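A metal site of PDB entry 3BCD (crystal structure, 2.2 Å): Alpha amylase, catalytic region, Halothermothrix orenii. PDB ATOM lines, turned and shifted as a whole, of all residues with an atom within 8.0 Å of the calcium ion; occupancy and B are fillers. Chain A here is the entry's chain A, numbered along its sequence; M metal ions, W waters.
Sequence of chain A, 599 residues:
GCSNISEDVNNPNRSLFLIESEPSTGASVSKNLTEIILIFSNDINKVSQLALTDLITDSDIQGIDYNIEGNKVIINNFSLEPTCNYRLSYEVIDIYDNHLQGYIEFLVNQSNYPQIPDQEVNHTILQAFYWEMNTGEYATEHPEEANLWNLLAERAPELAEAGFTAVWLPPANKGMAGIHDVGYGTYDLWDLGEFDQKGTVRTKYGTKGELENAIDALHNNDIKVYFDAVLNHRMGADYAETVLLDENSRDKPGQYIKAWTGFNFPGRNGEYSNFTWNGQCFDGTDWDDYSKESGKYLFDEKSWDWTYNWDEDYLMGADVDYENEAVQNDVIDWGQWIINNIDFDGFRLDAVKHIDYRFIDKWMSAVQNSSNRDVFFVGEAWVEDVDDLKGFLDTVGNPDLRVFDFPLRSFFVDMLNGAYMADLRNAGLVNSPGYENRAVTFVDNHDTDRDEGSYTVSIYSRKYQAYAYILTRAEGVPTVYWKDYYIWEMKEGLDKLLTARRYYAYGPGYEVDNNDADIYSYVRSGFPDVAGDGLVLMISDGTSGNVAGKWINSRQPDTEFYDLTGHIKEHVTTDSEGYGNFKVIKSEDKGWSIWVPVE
OD2 of Asp 400 lies within hydrogen-bond range of NE2 of Gln 368. NE2 of Gln 368 is in hydrogen-bond range of O of Val 375. The side-chain hydroxyl (OG) of Ser 371 lies within hydrogen-bond range of the backbone NH (N) of Arg 373, 3.0 Å away.
Within 4 Å of the calcium ion: Gln 368, Ser 371 and Arg 373.
The calcium ion is bound by the backbone carbonyl oxygen of Ser 371, the backbone carbonyl oxygen of Arg 373, water W2, the backbone carbonyl oxygen of Gln 368, water W1 and the side-chain amide oxygen of Gln 368. The calcium ion has six donor atoms within binding distance.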
ATOM      1  N   ILE A 339       9.188 -13.569  24.455  1.00  0.00           N
ATOM      2  CA  ILE A 339       8.043 -13.179  23.618  1.00  0.00           C
ATOM      3  C   ILE A 339       8.426 -12.415  22.350  1.00  0.00           C
ATOM      4  O   ILE A 339       8.100 -12.843  21.244  1.00  0.00           O
ATOM      5  CB  ILE A 339       7.025 -12.340  24.429  1.00  0.00           C
ATOM      6  CG1 ILE A 339       6.475 -13.182  25.588  1.00  0.00           C
ATOM      7  CG2 ILE A 339       5.826 -11.875  23.596  1.00  0.00           C
ATOM      8  CD1 ILE A 339       5.710 -14.338  25.185  1.00  0.00           C
ATOM      9  N   ASN A 340       9.068 -11.277  22.495  1.00  0.00           N
ATOM     10  CA  ASN A 340       9.263 -10.384  21.385  1.00  0.00           C
ATOM     11  C   ASN A 340      10.455 -10.703  20.519  1.00  0.00           C
ATOM     12  O   ASN A 340      10.487 -10.289  19.361  1.00  0.00           O
ATOM     13  CB  ASN A 340       9.410  -8.951  21.891  1.00  0.00           C
ATOM     14  CG  ASN A 340       8.186  -8.476  22.606  1.00  0.00           C
ATOM     15  OD1 ASN A 340       7.048  -8.722  22.164  1.00  0.00           O
ATOM     16  ND2 ASN A 340       8.389  -7.826  23.753  1.00  0.00           N
ATOM     17  N   MET A 364       4.073 -10.209  34.870  1.00  0.00           N
ATOM     18  CA  MET A 364       3.059 -10.527  33.886  1.00  0.00           C
ATOM     19  C   MET A 364       2.690  -9.237  33.167  1.00  0.00           C
ATOM     20  O   MET A 364       2.577  -9.208  31.947  1.00  0.00           O
ATOM     21  CB  MET A 364       1.832 -11.144  34.548  1.00  0.00           C
ATOM     22  CG  MET A 364       1.976 -12.623  34.961  1.00  0.00           C
ATOM     23  SD  MET A 364       0.389 -13.209  35.601  1.00  0.00           S
ATOM     24  CE  MET A 364      -0.867 -12.884  34.399  1.00  0.00           C
ATOM     25  N   SER A 365       2.506  -8.167  33.910  1.00  0.00           N
ATOM     26  CA  SER A 365       2.068  -6.890  33.311  1.00  0.00           C
ATOM     27  C   SER A 365       3.097  -6.274  32.405  1.00  0.00           C
ATOM     28  O   SER A 365       2.730  -5.687  31.360  1.00  0.00           O
ATOM     29  CB  SER A 365       1.725  -5.917  34.408  1.00  0.00           C
ATOM     30  OG  SER A 365       0.504  -6.356  35.007  1.00  0.00           O
ATOM     31  N   ALA A 366       4.375  -6.381  32.778  1.00  0.00           N
ATOM     32  CA  ALA A 366       5.446  -5.747  32.033  1.00  0.00           C
ATOM     33  C   ALA A 366       5.542  -6.492  30.727  1.00  0.00           C
ATOM     34  O   ALA A 366       5.540  -5.905  29.661  1.00  0.00           O
ATOM     35  CB  ALA A 366       6.808  -5.742  32.843  1.00  0.00           C
ATOM     36  N   VAL A 367       5.582  -7.816  30.802  1.00  0.00           N
ATOM     37  CA  VAL A 367       5.635  -8.667  29.587  1.00  0.00           C
ATOM     38  C   VAL A 367       4.418  -8.403  28.622  1.00  0.00           C
ATOM     39  O   VAL A 367       4.577  -8.067  27.434  1.00  0.00           O
ATOM     40  CB  VAL A 367       5.751 -10.165  30.027  1.00  0.00           C
ATOM     41  CG1 VAL A 367       5.526 -11.085  28.854  1.00  0.00           C
ATOM     42  CG2 VAL A 367       7.132 -10.473  30.740  1.00  0.00           C
ATOM     43  N   GLN A 368       3.208  -8.518  29.169  1.00  0.00           N
ATOM     44  CA  GLN A 368       2.008  -8.247  28.391  1.00  0.00           C
ATOM     45  C   GLN A 368       2.048  -6.834  27.692  1.00  0.00           C
ATOM     46  O   GLN A 368       1.914  -6.727  26.493  1.00  0.00           O
ATOM     47  CB  GLN A 368       0.765  -8.433  29.264  1.00  0.00           C
ATOM     48  CG  GLN A 368      -0.596  -8.328  28.548  1.00  0.00           C
ATOM     49  CD  GLN A 368      -0.845  -9.491  27.614  1.00  0.00           C
ATOM     50  OE1 GLN A 368      -0.424  -9.440  26.436  1.00  0.00           O
ATOM     51  NE2 GLN A 368      -1.575 -10.547  28.120  1.00  0.00           N
ATOM     52  N   ASN A 369       2.257  -5.780  28.453  1.00  0.00           N
ATOM     53  CA  ASN A 369       2.331  -4.411  27.897  1.00  0.00           C
ATOM     54  C   ASN A 369       3.422  -4.219  26.851  1.00  0.00           C
ATOM     55  O   ASN A 369       3.410  -3.219  26.121  1.00  0.00           O
ATOM     56  CB  ASN A 369       2.664  -3.446  29.057  1.00  0.00           C
ATOM     57  CG  ASN A 369       1.503  -3.214  29.986  1.00  0.00           C
ATOM     58  OD1 ASN A 369       0.381  -3.586  29.680  1.00  0.00           O
ATOM     59  ND2 ASN A 369       1.757  -2.557  31.132  1.00  0.00           N
ATOM     60  N   SER A 370       4.415  -5.115  26.847  1.00  0.00           N
ATOM     61  CA  SER A 370       5.571  -4.985  25.972  1.00  0.00           C
ATOM     62  C   SER A 370       5.266  -5.300  24.494  1.00  0.00           C
ATOM     63  O   SER A 370       6.050  -4.917  23.609  1.00  0.00           O
ATOM     64  CB  SER A 370       6.741  -5.886  26.433  1.00  0.00           C
ATOM     65  OG  SER A 370       6.749  -7.171  25.803  1.00  0.00           O
ATOM     66  N   SER A 371       4.201  -6.019  24.194  1.00  0.00           N
ATOM     67  CA  SER A 371       3.867  -6.287  22.799  1.00  0.00           C
ATOM     68  C   SER A 371       2.366  -6.237  22.602  1.00  0.00           C
ATOM     69  O   SER A 371       1.609  -6.309  23.582  1.00  0.00           O
ATOM     70  CB  SER A 371       4.461  -7.628  22.402  1.00  0.00           C
ATOM     71  OG  SER A 371       3.501  -8.505  21.787  1.00  0.00           O
ATOM     72  N   ASN A 372       1.917  -6.110  21.359  1.00  0.00           N
ATOM     73  CA  ASN A 372       0.475  -6.134  21.087  1.00  0.00           C
ATOM     74  C   ASN A 372      -0.184  -7.515  21.048  1.00  0.00           C
ATOM     75  O   ASN A 372      -1.392  -7.615  21.083  1.00  0.00           O
ATOM     76  CB  ASN A 372       0.182  -5.442  19.773  1.00  0.00           C
ATOM     77  CG  ASN A 372       0.472  -3.980  19.835  1.00  0.00           C
ATOM     78  OD1 ASN A 372       0.688  -3.426  20.909  1.00  0.00           O
ATOM     79  ND2 ASN A 372       0.463  -3.353  18.693  1.00  0.00           N
ATOM     80  N   ARG A 373       0.610  -8.564  20.955  1.00  0.00           N
ATOM     81  CA  ARG A 373       0.024  -9.874  21.018  1.00  0.00           C
ATOM     82  C   ARG A 373      -0.485 -10.078  22.414  1.00  0.00           C
ATOM     83  O   ARG A 373       0.107  -9.582  23.383  1.00  0.00           O
ATOM     84  CB  ARG A 373       1.007 -10.944  20.616  1.00  0.00           C
ATOM     85  CG  ARG A 373       1.434 -11.948  21.683  1.00  0.00           C
ATOM     86  CD  ARG A 373       2.365 -13.028  21.037  1.00  0.00           C
ATOM     87  NE  ARG A 373       3.447 -12.356  20.332  1.00  0.00           N
ATOM     88  CZ  ARG A 373       4.396 -12.935  19.611  1.00  0.00           C
ATOM     89  NH1 ARG A 373       5.308 -12.144  19.058  1.00  0.00           N
ATOM     90  NH2 ARG A 373       4.444 -14.256  19.462  1.00  0.00           N
ATOM     91  N   ASP A 374      -1.595 -10.808  22.525  1.00  0.00           N
ATOM     92  CA  ASP A 374      -2.255 -11.053  23.782  1.00  0.00           C
ATOM     93  C   ASP A 374      -1.606 -12.306  24.380  1.00  0.00           C
ATOM     94  O   ASP A 374      -1.947 -13.427  24.028  1.00  0.00           O
ATOM     95  CB  ASP A 374      -3.752 -11.228  23.500  1.00  0.00           C
ATOM     96  CG  ASP A 374      -4.585 -11.686  24.718  1.00  0.00           C
ATOM     97  OD1 ASP A 374      -4.111 -11.711  25.887  1.00  0.00           O
ATOM     98  OD2 ASP A 374      -5.770 -12.028  24.500  1.00  0.00           O
ATOM     99  N   VAL A 375      -0.645 -12.081  25.279  1.00  0.00           N
ATOM    100  CA  VAL A 375       0.112 -13.152  25.834  1.00  0.00           C
ATOM    101  C   VAL A 375      -0.757 -13.946  26.835  1.00  0.00           C
ATOM    102  O   VAL A 375      -1.684 -13.419  27.441  1.00  0.00           O
ATOM    103  CB  VAL A 375       1.446 -12.664  26.480  1.00  0.00           C
ATOM    104  CG1 VAL A 375       2.202 -13.859  27.054  1.00  0.00           C
ATOM    105  CG2 VAL A 375       2.342 -11.907  25.477  1.00  0.00           C
ATOM    106  N   PHE A 376      -0.425 -15.221  26.963  1.00  0.00           N
ATOM    107  CA  PHE A 376      -1.227 -16.233  27.677  1.00  0.00           C
ATOM    108  C   PHE A 376      -0.379 -16.770  28.803  1.00  0.00           C
ATOM    109  O   PHE A 376       0.745 -17.174  28.574  1.00  0.00           O
ATOM    110  CB  PHE A 376      -1.566 -17.382  26.713  1.00  0.00           C
ATOM    111  CG  PHE A 376      -2.217 -18.619  27.361  1.00  0.00           C
ATOM    112  CD1 PHE A 376      -3.535 -18.870  27.180  1.00  0.00           C
ATOM    113  CD2 PHE A 376      -1.466 -19.533  28.046  1.00  0.00           C
ATOM    114  CE1 PHE A 376      -4.145 -19.979  27.745  1.00  0.00           C
ATOM    115  CE2 PHE A 376      -2.058 -20.664  28.636  1.00  0.00           C
ATOM    116  CZ  PHE A 376      -3.422 -20.879  28.485  1.00  0.00           C
ATOM    117  N   PHE A 377      -0.978 -16.785  29.984  1.00  0.00           N
ATOM    118  CA  PHE A 377      -0.351 -17.176  31.250  1.00  0.00           C
ATOM    119  C   PHE A 377      -1.212 -18.227  32.026  1.00  0.00           C
ATOM    120  O   PHE A 377      -2.447 -18.057  32.199  1.00  0.00           O
ATOM    121  CB  PHE A 377      -0.199 -15.925  32.108  1.00  0.00           C
ATOM    122  CG  PHE A 377       0.635 -14.785  31.493  1.00  0.00           C
ATOM    123  CD1 PHE A 377       0.041 -13.666  30.998  1.00  0.00           C
ATOM    124  CD2 PHE A 377       2.039 -14.813  31.517  1.00  0.00           C
ATOM    125  CE1 PHE A 377       0.813 -12.633  30.502  1.00  0.00           C
ATOM    126  CE2 PHE A 377       2.768 -13.769  31.032  1.00  0.00           C
ATOM    127  CZ  PHE A 377       2.144 -12.702  30.544  1.00  0.00           C
ATOM    128  N   ASP A 400      -5.050 -11.606  33.920  1.00  0.00           N
ATOM    129  CA  ASP A 400      -4.549 -12.482  32.857  1.00  0.00           C
ATOM    130  C   ASP A 400      -4.199 -13.858  33.364  1.00  0.00           C
ATOM    131  O   ASP A 400      -4.051 -14.770  32.541  1.00  0.00           O
ATOM    132  CB  ASP A 400      -3.356 -11.911  32.089  1.00  0.00           C
ATOM    133  CG  ASP A 400      -3.722 -10.751  31.114  1.00  0.00           C
ATOM    134  OD1 ASP A 400      -4.920 -10.527  30.760  1.00  0.00           O
ATOM    135  OD2 ASP A 400      -2.749 -10.085  30.654  1.00  0.00           O
HETATM  136 CA    CA M   1       0.622  -7.922  24.947  1.00  0.00          CA
HETATM  137  O   HOH W   1       2.891  -8.534  24.744  1.00  0.00           O
HETATM  138  O   HOH W   2      -0.511  -5.884  25.136  1.00  0.00           O
